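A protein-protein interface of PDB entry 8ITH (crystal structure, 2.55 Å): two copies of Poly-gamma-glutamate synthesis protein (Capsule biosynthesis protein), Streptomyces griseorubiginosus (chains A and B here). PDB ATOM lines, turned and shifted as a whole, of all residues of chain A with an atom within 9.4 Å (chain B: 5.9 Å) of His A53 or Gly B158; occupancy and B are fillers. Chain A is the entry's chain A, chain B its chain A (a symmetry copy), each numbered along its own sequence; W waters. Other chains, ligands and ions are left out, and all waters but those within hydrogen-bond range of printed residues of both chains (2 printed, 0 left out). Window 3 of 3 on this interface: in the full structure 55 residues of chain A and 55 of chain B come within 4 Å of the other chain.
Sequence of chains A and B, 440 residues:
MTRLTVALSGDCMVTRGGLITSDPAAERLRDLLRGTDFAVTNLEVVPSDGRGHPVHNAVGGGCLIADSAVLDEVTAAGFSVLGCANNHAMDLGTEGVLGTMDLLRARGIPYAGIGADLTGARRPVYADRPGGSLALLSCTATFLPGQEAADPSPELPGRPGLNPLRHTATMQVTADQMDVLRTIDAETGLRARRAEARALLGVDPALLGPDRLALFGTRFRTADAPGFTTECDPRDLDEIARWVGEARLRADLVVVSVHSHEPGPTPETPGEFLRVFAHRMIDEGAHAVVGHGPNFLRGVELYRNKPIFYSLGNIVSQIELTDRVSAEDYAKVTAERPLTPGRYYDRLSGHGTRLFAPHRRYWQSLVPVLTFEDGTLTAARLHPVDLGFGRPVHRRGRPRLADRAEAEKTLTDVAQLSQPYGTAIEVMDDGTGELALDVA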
ATOM      1  N   VAL A  46       7.982 -23.710 -23.904  1.00  0.00           N
ATOM      2  CA  VAL A  46       7.455 -22.407 -24.301  1.00  0.00           C
ATOM      3  C   VAL A  46       7.699 -22.246 -25.798  1.00  0.00           C
ATOM      4  O   VAL A  46       8.858 -22.070 -26.209  1.00  0.00           O
ATOM      5  CB  VAL A  46       8.111 -21.266 -23.511  1.00  0.00           C
ATOM      6  CG1 VAL A  46       7.499 -19.930 -23.912  1.00  0.00           C
ATOM      7  CG2 VAL A  46       7.955 -21.490 -22.025  1.00  0.00           C
ATOM      8  N   SER A  48       7.935 -19.955 -28.924  1.00  0.00           N
ATOM      9  CA  SER A  48       8.277 -18.545 -28.896  1.00  0.00           C
ATOM     10  C   SER A  48       8.622 -18.050 -30.290  1.00  0.00           C
ATOM     11  O   SER A  48       9.185 -18.780 -31.108  1.00  0.00           O
ATOM     12  CB  SER A  48       9.451 -18.280 -27.943  1.00  0.00           C
ATOM     13  OG  SER A  48       9.713 -16.892 -27.831  1.00  0.00           O
ATOM     14  N   GLY A  50       9.968 -14.777 -29.969  1.00  0.00           N
ATOM     15  CA  GLY A  50      10.912 -13.786 -29.491  1.00  0.00           C
ATOM     16  C   GLY A  50      10.429 -12.974 -28.305  1.00  0.00           C
ATOM     17  O   GLY A  50      11.207 -12.229 -27.702  1.00  0.00           O
ATOM     18  N   ARG A  51       9.153 -13.112 -27.954  1.00  0.00           N
ATOM     19  CA  ARG A  51       8.567 -12.301 -26.894  1.00  0.00           C
ATOM     20  C   ARG A  51       8.902 -12.884 -25.526  1.00  0.00           C
ATOM     21  O   ARG A  51       8.759 -14.090 -25.301  1.00  0.00           O
ATOM     22  CB  ARG A  51       7.052 -12.210 -27.076  1.00  0.00           C
ATOM     23  CG  ARG A  51       6.360 -11.275 -26.103  1.00  0.00           C
ATOM     24  CD  ARG A  51       4.864 -11.212 -26.375  1.00  0.00           C
ATOM     25  NE  ARG A  51       4.190 -10.257 -25.501  1.00  0.00           N
ATOM     26  CZ  ARG A  51       2.877 -10.055 -25.489  1.00  0.00           C
ATOM     27  NH1 ARG A  51       2.353  -9.164 -24.658  1.00  0.00           N
ATOM     28  NH2 ARG A  51       2.087 -10.743 -26.304  1.00  0.00           N
ATOM     29  N   GLY A  52       9.343 -12.026 -24.616  1.00  0.00           N
ATOM     30  CA  GLY A  52       9.650 -12.421 -23.256  1.00  0.00           C
ATOM     31  C   GLY A  52      11.142 -12.360 -22.970  1.00  0.00           C
ATOM     32  O   GLY A  52      11.962 -12.000 -23.817  1.00  0.00           O
ATOM     33  N   HIS A  53      11.476 -12.722 -21.732  1.00  0.00           N
ATOM     34  CA  HIS A  53      12.847 -12.752 -21.251  1.00  0.00           C
ATOM     35  C   HIS A  53      13.024 -13.998 -20.394  1.00  0.00           C
ATOM     36  O   HIS A  53      12.107 -14.370 -19.648  1.00  0.00           O
ATOM     37  CB  HIS A  53      13.193 -11.498 -20.435  1.00  0.00           C
ATOM     38  CG  HIS A  53      12.888 -10.213 -21.141  1.00  0.00           C
ATOM     39  ND1 HIS A  53      13.772  -9.612 -22.013  1.00  0.00           N
ATOM     40  CD2 HIS A  53      11.796  -9.413 -21.104  1.00  0.00           C
ATOM     41  CE1 HIS A  53      13.236  -8.499 -22.483  1.00  0.00           C
ATOM     42  NE2 HIS A  53      12.038  -8.356 -21.947  1.00  0.00           N
ATOM     43  N   PRO A  54      14.178 -14.657 -20.472  1.00  0.00           N
ATOM     44  CA  PRO A  54      14.359 -15.903 -19.718  1.00  0.00           C
ATOM     45  C   PRO A  54      14.365 -15.645 -18.221  1.00  0.00           C
ATOM     46  O   PRO A  54      14.987 -14.695 -17.733  1.00  0.00           O
ATOM     47  CB  PRO A  54      15.721 -16.423 -20.198  1.00  0.00           C
ATOM     48  CG  PRO A  54      16.085 -15.585 -21.394  1.00  0.00           C
ATOM     49  CD  PRO A  54      15.394 -14.275 -21.205  1.00  0.00           C
ATOM     50  N   VAL A  55      13.657 -16.498 -17.491  1.00  0.00           N
ATOM     51  CA  VAL A  55      13.672 -16.463 -16.040  1.00  0.00           C
ATOM     52  C   VAL A  55      14.679 -17.494 -15.551  1.00  0.00           C
ATOM     53  O   VAL A  55      15.011 -18.462 -16.242  1.00  0.00           O
ATOM     54  CB  VAL A  55      12.272 -16.714 -15.435  1.00  0.00           C
ATOM     55  CG1 VAL A  55      11.244 -15.788 -16.076  1.00  0.00           C
ATOM     56  CG2 VAL A  55      11.867 -18.172 -15.601  1.00  0.00           C
ATOM     57  N   HIS A  56      15.188 -17.280 -14.342  1.00  0.00           N
ATOM     58  CA  HIS A  56      16.162 -18.197 -13.758  1.00  0.00           C
ATOM     59  C   HIS A  56      15.413 -19.382 -13.161  1.00  0.00           C
ATOM     60  O   HIS A  56      14.845 -19.291 -12.070  1.00  0.00           O
ATOM     61  CB  HIS A  56      17.011 -17.490 -12.709  1.00  0.00           C
ATOM     62  CG  HIS A  56      18.139 -18.324 -12.189  1.00  0.00           C
ATOM     63  ND1 HIS A  56      18.907 -17.948 -11.108  1.00  0.00           N
ATOM     64  CD2 HIS A  56      18.630 -19.517 -12.603  1.00  0.00           C
ATOM     65  CE1 HIS A  56      19.820 -18.874 -10.878  1.00  0.00           C
ATOM     66  NE2 HIS A  56      19.674 -19.836 -11.771  1.00  0.00           N
ATOM     67  N   ASN A  57      15.410 -20.497 -13.882  1.00  0.00           N
ATOM     68  CA  ASN A  57      14.730 -21.718 -13.461  1.00  0.00           C
ATOM     69  C   ASN A  57      15.764 -22.834 -13.339  1.00  0.00           C
ATOM     70  O   ASN A  57      15.738 -23.807 -14.096  1.00  0.00           O
ATOM     71  CB  ASN A  57      13.613 -22.087 -14.456  1.00  0.00           C
ATOM     72  CG  ASN A  57      12.762 -23.249 -13.979  1.00  0.00           C
ATOM     73  OD1 ASN A  57      12.795 -23.619 -12.806  1.00  0.00           O
ATOM     74  ND2 ASN A  57      11.990 -23.829 -14.892  1.00  0.00           N
ATOM     75  N   CYS A  63      15.966 -23.450 -18.780  1.00  0.00           N
ATOM     76  CA  CYS A  63      14.878 -22.953 -19.608  1.00  0.00           C
ATOM     77  C   CYS A  63      14.574 -23.935 -20.732  1.00  0.00           C
ATOM     78  O   CYS A  63      15.463 -24.609 -21.260  1.00  0.00           O
ATOM     79  CB  CYS A  63      15.223 -21.581 -20.189  1.00  0.00           C
ATOM     80  SG  CYS A  63      15.152 -20.231 -18.995  1.00  0.00           S
ATOM     81  N   ILE A  65      12.696 -23.555 -24.107  1.00  0.00           N
ATOM     82  CA  ILE A  65      12.115 -22.658 -25.098  1.00  0.00           C
ATOM     83  C   ILE A  65      12.418 -23.215 -26.480  1.00  0.00           C
ATOM     84  O   ILE A  65      13.528 -23.698 -26.730  1.00  0.00           O
ATOM     85  CB  ILE A  65      12.672 -21.228 -24.951  1.00  0.00           C
ATOM     86  CG1 ILE A  65      12.554 -20.763 -23.498  1.00  0.00           C
ATOM     87  CG2 ILE A  65      11.955 -20.270 -25.890  1.00  0.00           C
ATOM     88  CD1 ILE A  65      13.461 -19.610 -23.155  1.00  0.00           C
ATOM     89  N   HIS A  88       7.398 -25.019 -16.495  1.00  0.00           N
ATOM     90  CA  HIS A  88       8.153 -24.394 -17.569  1.00  0.00           C
ATOM     91  C   HIS A  88       7.365 -23.367 -18.366  1.00  0.00           C
ATOM     92  O   HIS A  88       7.969 -22.639 -19.159  1.00  0.00           O
ATOM     93  CB  HIS A  88       8.702 -25.454 -18.535  1.00  0.00           C
ATOM     94  CG  HIS A  88       9.912 -26.167 -18.021  1.00  0.00           C
ATOM     95  ND1 HIS A  88      11.149 -25.562 -17.935  1.00  0.00           N
ATOM     96  CD2 HIS A  88      10.078 -27.430 -17.563  1.00  0.00           C
ATOM     97  CE1 HIS A  88      12.022 -26.424 -17.443  1.00  0.00           C
ATOM     98  NE2 HIS A  88      11.399 -27.564 -17.210  1.00  0.00           N
ATOM     99  N   ALA A  89       6.044 -23.275 -18.175  1.00  0.00           N
ATOM    100  CA  ALA A  89       5.244 -22.345 -18.966  1.00  0.00           C
ATOM    101  C   ALA A  89       5.689 -20.901 -18.773  1.00  0.00           C
ATOM    102  O   ALA A  89       5.524 -20.076 -19.678  1.00  0.00           O
ATOM    103  CB  ALA A  89       3.765 -22.489 -18.610  1.00  0.00           C
ATOM    104  N   MET A  90       6.255 -20.577 -17.610  1.00  0.00           N
ATOM    105  CA  MET A  90       6.690 -19.221 -17.302  1.00  0.00           C
ATOM    106  C   MET A  90       8.176 -19.006 -17.571  1.00  0.00           C
ATOM    107  O   MET A  90       8.768 -18.074 -17.016  1.00  0.00           O
ATOM    108  CB  MET A  90       6.366 -18.880 -15.846  1.00  0.00           C
ATOM    109  CG  MET A  90       4.882 -18.842 -15.532  1.00  0.00           C
ATOM    110  SD  MET A  90       4.019 -17.584 -16.490  1.00  0.00           S
ATOM    111  CE  MET A  90       4.776 -16.100 -15.834  1.00  0.00           C
ATOM    112  N   ASP A  91       8.791 -19.841 -18.413  1.00  0.00           N
ATOM    113  CA  ASP A  91      10.230 -19.744 -18.636  1.00  0.00           C
ATOM    114  C   ASP A  91      10.631 -18.444 -19.319  1.00  0.00           C
ATOM    115  O   ASP A  91      11.779 -18.012 -19.168  1.00  0.00           O
ATOM    116  CB  ASP A  91      10.727 -20.940 -19.450  1.00  0.00           C
ATOM    117  CG  ASP A  91      11.082 -22.131 -18.577  1.00  0.00           C
ATOM    118  OD1 ASP A  91      10.858 -22.058 -17.349  1.00  0.00           O
ATOM    119  OD2 ASP A  91      11.593 -23.137 -19.111  1.00  0.00           O
ATOM    120  N   LEU A  92       9.723 -17.810 -20.061  1.00  0.00           N
ATOM    121  CA  LEU A  92       9.977 -16.501 -20.650  1.00  0.00           C
ATOM    122  C   LEU A  92       9.204 -15.393 -19.943  1.00  0.00           C
ATOM    123  O   LEU A  92       9.013 -14.316 -20.515  1.00  0.00           O
ATOM    124  CB  LEU A  92       9.648 -16.511 -22.142  1.00  0.00           C
ATOM    125  CG  LEU A  92      10.713 -17.135 -23.047  1.00  0.00           C
ATOM    126  CD1 LEU A  92      10.219 -17.197 -24.482  1.00  0.00           C
ATOM    127  CD2 LEU A  92      12.009 -16.345 -22.964  1.00  0.00           C
ATOM    128  N   GLY A  93       8.754 -15.638 -18.711  1.00  0.00           N
ATOM    129  CA  GLY A  93       8.072 -14.626 -17.932  1.00  0.00           C
ATOM    130  C   GLY A  93       6.633 -14.393 -18.362  1.00  0.00           C
ATOM    131  O   GLY A  93       6.051 -15.132 -19.164  1.00  0.00           O
ATOM    132  N   THR A  94       6.052 -13.328 -17.797  1.00  0.00           N
ATOM    133  CA  THR A  94       4.667 -12.984 -18.109  1.00  0.00           C
ATOM    134  C   THR A  94       4.499 -12.624 -19.579  1.00  0.00           C
ATOM    135  O   THR A  94       3.453 -12.912 -20.172  1.00  0.00           O
ATOM    136  CB  THR A  94       4.193 -11.825 -17.227  1.00  0.00           C
ATOM    137  OG1 THR A  94       4.989 -10.665 -17.493  1.00  0.00           O
ATOM    138  CG2 THR A  94       4.319 -12.183 -15.757  1.00  0.00           C
ATOM    139  N   GLU A  95       5.505 -11.987 -20.182  1.00  0.00           N
ATOM    140  CA  GLU A  95       5.423 -11.687 -21.607  1.00  0.00           C
ATOM    141  C   GLU A  95       5.474 -12.956 -22.444  1.00  0.00           C
ATOM    142  O   GLU A  95       4.823 -13.034 -23.494  1.00  0.00           O
ATOM    143  CB  GLU A  95       6.547 -10.736 -22.015  1.00  0.00           C
ATOM    144  CG  GLU A  95       6.314  -9.289 -21.618  1.00  0.00           C
ATOM    145  CD  GLU A  95       5.044  -8.721 -22.220  1.00  0.00           C
ATOM    146  OE1 GLU A  95       4.037  -8.602 -21.489  1.00  0.00           O
ATOM    147  OE2 GLU A  95       5.053  -8.405 -23.429  1.00  0.00           O
ATOM    148  N   GLY A  96       6.237 -13.956 -21.999  1.00  0.00           N
ATOM    149  CA  GLY A  96       6.301 -15.207 -22.734  1.00  0.00           C
ATOM    150  C   GLY A  96       4.991 -15.969 -22.703  1.00  0.00           C
ATOM    151  O   GLY A  96       4.559 -16.520 -23.718  1.00  0.00           O
ATOM    152  N   VAL A  97       4.335 -16.008 -21.539  1.00  0.00           N
ATOM    153  CA  VAL A  97       3.076 -16.739 -21.445  1.00  0.00           C
ATOM    154  C   VAL A  97       1.975 -16.015 -22.217  1.00  0.00           C
ATOM    155  O   VAL A  97       1.057 -16.654 -22.745  1.00  0.00           O
ATOM    156  CB  VAL A  97       2.697 -16.973 -19.968  1.00  0.00           C
ATOM    157  CG1 VAL A  97       2.164 -15.705 -19.328  1.00  0.00           C
ATOM    158  CG2 VAL A  97       1.692 -18.103 -19.847  1.00  0.00           C
ATOM    159  N   GLN A 147       5.002 -17.324  -9.789  1.00  0.00           N
ATOM    160  CA  GLN A 147       4.632 -17.608 -11.171  1.00  0.00           C
ATOM    161  C   GLN A 147       3.138 -17.849 -11.338  1.00  0.00           C
ATOM    162  O   GLN A 147       2.644 -17.815 -12.470  1.00  0.00           O
ATOM    163  CB  GLN A 147       5.414 -18.815 -11.691  1.00  0.00           C
ATOM    164  CG  GLN A 147       6.887 -18.534 -11.941  1.00  0.00           C
ATOM    165  CD  GLN A 147       7.601 -19.694 -12.611  1.00  0.00           C
ATOM    166  OE1 GLN A 147       7.169 -20.844 -12.518  1.00  0.00           O
ATOM    167  NE2 GLN A 147       8.700 -19.394 -13.297  1.00  0.00           N
ATOM    168  N   VAL A 325      19.644 -21.639 -24.913  1.00  0.00           N
ATOM    169  CA  VAL A 325      20.202 -21.804 -23.574  1.00  0.00           C
ATOM    170  C   VAL A 325      20.518 -20.420 -23.024  1.00  0.00           C
ATOM    171  O   VAL A 325      21.262 -19.652 -23.645  1.00  0.00           O
ATOM    172  CB  VAL A 325      21.451 -22.698 -23.584  1.00  0.00           C
ATOM    173  CG1 VAL A 325      22.085 -22.745 -22.202  1.00  0.00           C
ATOM    174  CG2 VAL A 325      21.092 -24.100 -24.053  1.00  0.00           C
ATOM    175  N   SER A 326      19.954 -20.103 -21.861  1.00  0.00           N
ATOM    176  CA  SER A 326      20.124 -18.780 -21.280  1.00  0.00           C
ATOM    177  C   SER A 326      21.507 -18.640 -20.647  1.00  0.00           C
ATOM    178  O   SER A 326      22.217 -19.622 -20.411  1.00  0.00           O
ATOM    179  CB  SER A 326      19.043 -18.505 -20.233  1.00  0.00           C
ATOM    180  OG  SER A 326      19.327 -19.180 -19.018  1.00  0.00           O
ATOM    181  N   ALA A 327      21.880 -17.388 -20.365  1.00  0.00           N
ATOM    182  CA  ALA A 327      23.193 -17.116 -19.788  1.00  0.00           C
ATOM    183  C   ALA A 327      23.321 -17.706 -18.390  1.00  0.00           C
ATOM    184  O   ALA A 327      24.382 -18.227 -18.026  1.00  0.00           O
ATOM    185  CB  ALA A 327      23.452 -15.610 -19.755  1.00  0.00           C
ATOM    186  N   GLU A 328      22.258 -17.624 -17.589  1.00  0.00           N
ATOM    187  CA  GLU A 328      22.299 -18.207 -16.252  1.00  0.00           C
ATOM    188  C   GLU A 328      22.418 -19.726 -16.318  1.00  0.00           C
ATOM    189  O   GLU A 328      23.098 -20.337 -15.484  1.00  0.00           O
ATOM    190  CB  GLU A 328      21.057 -17.790 -15.464  1.00  0.00           C
ATOM    191  CG  GLU A 328      21.021 -16.305 -15.118  1.00  0.00           C
ATOM    192  CD  GLU A 328      19.657 -15.841 -14.646  1.00  0.00           C
ATOM    193  OE1 GLU A 328      18.654 -16.155 -15.321  1.00  0.00           O
ATOM    194  OE2 GLU A 328      19.586 -15.166 -13.596  1.00  0.00           O
ATOM    195  N   THR B  94       9.146  -7.226 -14.994  1.00  0.00           N
ATOM    196  CA  THR B  94      10.134  -6.776 -15.972  1.00  0.00           C
ATOM    197  C   THR B  94       9.574  -5.680 -16.868  1.00  0.00           C
ATOM    198  O   THR B  94      10.311  -4.777 -17.277  1.00  0.00           O
ATOM    199  CB  THR B  94      10.617  -7.955 -16.823  1.00  0.00           C
ATOM    200  OG1 THR B  94       9.514  -8.501 -17.554  1.00  0.00           O
ATOM    201  CG2 THR B  94      11.214  -9.041 -15.946  1.00  0.00           C
ATOM    202  N   GLU B  95       8.281  -5.745 -17.196  1.00  0.00           N
ATOM    203  CA  GLU B  95       7.680  -4.679 -17.990  1.00  0.00           C
ATOM    204  C   GLU B  95       7.612  -3.377 -17.208  1.00  0.00           C
ATOM    205  O   GLU B  95       7.762  -2.295 -17.790  1.00  0.00           O
ATOM    206  CB  GLU B  95       6.286  -5.090 -18.461  1.00  0.00           C
ATOM    207  CG  GLU B  95       6.282  -6.065 -19.625  1.00  0.00           C
ATOM    208  CD  GLU B  95       6.991  -5.512 -20.845  1.00  0.00           C
ATOM    209  OE1 GLU B  95       8.144  -5.921 -21.104  1.00  0.00           O
ATOM    210  OE2 GLU B  95       6.398  -4.658 -21.537  1.00  0.00           O
ATOM    211  N   LEU B  98      11.095  -1.765 -17.148  1.00  0.00           N
ATOM    212  CA  LEU B  98      11.348  -1.148 -18.444  1.00  0.00           C
ATOM    213  C   LEU B  98      10.541   0.135 -18.610  1.00  0.00           C
ATOM    214  O   LEU B  98      11.001   1.077 -19.266  1.00  0.00           O
ATOM    215  CB  LEU B  98      11.030  -2.131 -19.571  1.00  0.00           C
ATOM    216  CG  LEU B  98      12.020  -3.273 -19.801  1.00  0.00           C
ATOM    217  CD1 LEU B  98      11.450  -4.285 -20.779  1.00  0.00           C
ATOM    218  CD2 LEU B  98      13.340  -2.734 -20.314  1.00  0.00           C
ATOM    219  N   ALA B 116      18.016  -3.080 -18.616  1.00  0.00           N
ATOM    220  CA  ALA B 116      17.445  -4.103 -19.482  1.00  0.00           C
ATOM    221  C   ALA B 116      18.155  -5.440 -19.331  1.00  0.00           C
ATOM    222  O   ALA B 116      17.558  -6.481 -19.626  1.00  0.00           O
ATOM    223  CB  ALA B 116      17.496  -3.646 -20.938  1.00  0.00           C
ATOM    224  N   ASP B 117      19.413  -5.435 -18.886  1.00  0.00           N
ATOM    225  CA  ASP B 117      20.149  -6.655 -18.586  1.00  0.00           C
ATOM    226  C   ASP B 117      21.008  -6.413 -17.350  1.00  0.00           C
ATOM    227  O   ASP B 117      20.993  -5.326 -16.763  1.00  0.00           O
ATOM    228  CB  ASP B 117      20.982  -7.120 -19.792  1.00  0.00           C
ATOM    229  CG  ASP B 117      21.914  -6.043 -20.323  1.00  0.00           C
ATOM    230  OD1 ASP B 117      22.183  -5.054 -19.609  1.00  0.00           O
ATOM    231  OD2 ASP B 117      22.381  -6.192 -21.474  1.00  0.00           O
ATOM    232  N   ALA B 150      19.544 -10.151 -15.701  1.00  0.00           N
ATOM    233  CA  ALA B 150      20.349 -11.199 -16.307  1.00  0.00           C
ATOM    234  C   ALA B 150      20.954 -10.688 -17.603  1.00  0.00           C
ATOM    235  O   ALA B 150      20.329  -9.916 -18.335  1.00  0.00           O
ATOM    236  CB  ALA B 150      19.520 -12.463 -16.576  1.00  0.00           C
ATOM    237  N   ASP B 151      22.176 -11.120 -17.876  1.00  0.00           N
ATOM    238  CA  ASP B 151      22.865 -10.768 -19.106  1.00  0.00           C
ATOM    239  C   ASP B 151      22.466 -11.714 -20.230  1.00  0.00           C
ATOM    240  O   ASP B 151      21.987 -12.825 -19.984  1.00  0.00           O
ATOM    241  CB  ASP B 151      24.375 -10.808 -18.890  1.00  0.00           C
ATOM    242  CG  ASP B 151      24.936  -9.459 -18.482  1.00  0.00           C
ATOM    243  OD1 ASP B 151      24.304  -8.430 -18.808  1.00  0.00           O
ATOM    244  OD2 ASP B 151      26.006  -9.426 -17.840  1.00  0.00           O
ATOM    245  N   PRO B 152      22.636 -11.295 -21.482  1.00  0.00           N
ATOM    246  CA  PRO B 152      22.251 -12.160 -22.602  1.00  0.00           C
ATOM    247  C   PRO B 152      23.225 -13.311 -22.798  1.00  0.00           C
ATOM    248  O   PRO B 152      24.365 -13.300 -22.327  1.00  0.00           O
ATOM    249  CB  PRO B 152      22.275 -11.217 -23.814  1.00  0.00           C
ATOM    250  CG  PRO B 152      22.340  -9.828 -23.245  1.00  0.00           C
ATOM    251  CD  PRO B 152      23.042  -9.955 -21.937  1.00  0.00           C
ATOM    252  N   SER B 153      22.744 -14.320 -23.504  1.00  0.00           N
ATOM    253  CA  SER B 153      23.527 -15.428 -24.021  1.00  0.00           C
ATOM    254  C   SER B 153      23.612 -15.308 -25.540  1.00  0.00           C
ATOM    255  O   SER B 153      22.977 -14.435 -26.140  1.00  0.00           O
ATOM    256  CB  SER B 153      22.883 -16.762 -23.615  1.00  0.00           C
ATOM    257  OG  SER B 153      21.728 -17.033 -24.391  1.00  0.00           O
ATOM    258  N   LEU B 156      19.776 -16.250 -26.340  1.00  0.00           N
ATOM    259  CA  LEU B 156      18.629 -15.656 -25.678  1.00  0.00           C
ATOM    260  C   LEU B 156      18.990 -14.279 -25.146  1.00  0.00           C
ATOM    261  O   LEU B 156      20.150 -14.022 -24.809  1.00  0.00           O
ATOM    262  CB  LEU B 156      18.134 -16.540 -24.522  1.00  0.00           C
ATOM    263  CG  LEU B 156      17.422 -17.834 -24.922  1.00  0.00           C
ATOM    264  CD1 LEU B 156      17.142 -18.683 -23.694  1.00  0.00           C
ATOM    265  CD2 LEU B 156      16.134 -17.529 -25.679  1.00  0.00           C
ATOM    266  N   PRO B 157      18.021 -13.371 -25.064  1.00  0.00           N
ATOM    267  CA  PRO B 157      18.287 -12.057 -24.472  1.00  0.00           C
ATOM    268  C   PRO B 157      18.476 -12.169 -22.968  1.00  0.00           C
ATOM    269  O   PRO B 157      18.248 -13.212 -22.351  1.00  0.00           O
ATOM    270  CB  PRO B 157      17.029 -11.253 -24.814  1.00  0.00           C
ATOM    271  CG  PRO B 157      15.954 -12.291 -24.904  1.00  0.00           C
ATOM    272  CD  PRO B 157      16.620 -13.502 -25.506  1.00  0.00           C
ATOM    273  N   GLY B 158      18.909 -11.064 -22.374  1.00  0.00           N
ATOM    274  CA  GLY B 158      18.981 -10.989 -20.935  1.00  0.00           C
ATOM    275  C   GLY B 158      17.590 -10.829 -20.342  1.00  0.00           C
ATOM    276  O   GLY B 158      16.570 -11.043 -20.996  1.00  0.00           O
ATOM    277  N   ARG B 159      17.556 -10.436 -19.069  1.00  0.00           N
ATOM    278  CA  ARG B 159      16.298 -10.200 -18.379  1.00  0.00           C
ATOM    279  C   ARG B 159      16.380  -8.860 -17.657  1.00  0.00           C
ATOM    280  O   ARG B 159      17.356  -8.607 -16.923  1.00  0.00           O
ATOM    281  CB  ARG B 159      15.984 -11.333 -17.387  1.00  0.00           C
ATOM    282  CG  ARG B 159      14.699 -11.124 -16.595  1.00  0.00           C
ATOM    283  CD  ARG B 159      14.409 -12.277 -15.636  1.00  0.00           C
ATOM    284  NE  ARG B 159      15.422 -12.411 -14.591  1.00  0.00           N
ATOM    285  CZ  ARG B 159      16.373 -13.340 -14.584  1.00  0.00           C
ATOM    286  NH1 ARG B 159      16.447 -14.235 -15.566  1.00  0.00           N
ATOM    287  NH2 ARG B 159      17.249 -13.382 -13.588  1.00  0.00           N
ATOM    288  N   PRO B 160      15.406  -7.969 -17.847  1.00  0.00           N
ATOM    289  CA  PRO B 160      15.392  -6.723 -17.070  1.00  0.00           C
ATOM    290  C   PRO B 160      15.263  -7.015 -15.584  1.00  0.00           C
ATOM    291  O   PRO B 160      14.583  -7.959 -15.177  1.00  0.00           O
ATOM    292  CB  PRO B 160      14.165  -5.984 -17.610  1.00  0.00           C
ATOM    293  CG  PRO B 160      13.939  -6.554 -18.967  1.00  0.00           C
ATOM    294  CD  PRO B 160      14.344  -7.996 -18.866  1.00  0.00           C
HETATM  295  O   HOH W   1      20.031 -14.560 -20.667  1.00  0.00           O
HETATM  296  O   HOH W   2      13.830 -14.817 -12.822  1.00  0.00           O
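Glu A95 touches its own counterpart, Glu B95.
2 positions are printed for both chains.
Water W1 lies within hydrogen-bond range of the backbone carbonyl oxygen (O) of Asp B151 (2.7 Å), the backbone carbonyl oxygen (O) of Pro B157 (2.8 Å) and the backbone NH (N) of Ala A327 (3.4 Å).
Water W2 bridges N of His A56 (3.2 Å) and NE of Arg B159 (3.4 Å).
The guanidinium group of Arg A51 is in salt-bridge range of the side-chain carboxylate of Glu A95, at 2.9 Å.
N of His A53 is in hydrogen-bond range of O of Leu A92.
O of Val A55 is in hydrogen-bond range of SG of Cys A63, at 3.3 Å.
The backbone NH (N) of Val A55 lies within hydrogen-bond range of the backbone carbonyl oxygen (O) of Asp A91, at 2.9 Å.
OG of Ser B153 sits at hydrogen-bond distance from N of Leu B156.
O of Gly B158 sits at hydrogen-bond distance from ND1 of His A53 (3.3 Å).
The backbone carbonyl oxygen of Pro A54 is in hydrogen-bond range of the guanidinium group of Arg B159 (2.7 Å).
The backbone carbonyl oxygen (O) of Val A325 is in hydrogen-bond range of the side-chain hydroxyl (OG) of Ser B153.
The side-chain carboxylate of Glu A328 is in salt-bridge range of the guanidinium group of Arg B159 (2.9 Å).
Among the printed residues, pairs that only touch across the chains: His A53 with Arg B159 (3.9 Å), His A53 with Pro B160 (3.5 Å), Pro A54 with Leu B156 (3.9 Å), Pro A54 with Pro B157 (3.3 Å), Pro A54 with Gly B158 (3.4 Å), Val A55 with Arg B159 (3.6 Å), His A56 with Arg B159 (3.5 Å), Ile A65 with Leu B156 (3.8 Å), Glu A95 with Glu B95 (3.8 Å), Val A325 with Leu B156 (3.9 Å), Ser A326 with Ser B153 (3.8 Å), Ser A326 with Leu B156 (3.6 Å), Ala A327 with Asp B151 (3.2 Å), Ala A327 with Pro B152 (3.6 Å), Ala A327 with Ser B153 (3.5 Å) and Glu A328 with Ala B150 (3.9 Å).
Of the 27 printed residues of chain A, 10 touch a printed residue of chain B.
Hydrophobic or aromatic side chains of chain A that line the printed part of chain B: His A53, Pro A54, Ile A65 and Ala A327.
Of the 14 printed residues of chain B, 10 touch a printed residue of chain A.
Hydrophobic or aromatic side chains of chain B that line the printed part of chain A: Ala B150, Leu B156 and Pro B160.
Among the printed residues, 20 pairs touch across the chains.
Among the printed residues, Asp or Glu carboxylates within 4 Å of a Lys or Arg side-chain nitrogen of the other chain: Glu A328 with Arg B159 (2.9 Å).
Arg A51 touches none of the printed residues of chain B.
Of the printed residues of chain B, His A53 touches Gly B158 (3.3 Å), Arg B159 (3.9 Å) and Pro B160 (3.5 Å).
Printed residues of chain B within 4 Å of Val A55: Arg B159.
Of the printed residues of chain B, Glu A95 touches Glu B95 (3.8 Å).
Gln A147 touches none of the printed residues of chain B.
Of the printed residues of chain B, Ser A326 touches Ser B153 and Leu B156.
Printed residues of chain A within 4 Å of Glu B95: Glu A95 (3.8 Å).
Pro B157 touches just one residue of chain A: Pro A54 (3.3 Å).
Gly B158 touches two residues of chain A.
The nearest residue of chain A that does not touch Gly B158 is Gly A52 (5.5 Å).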
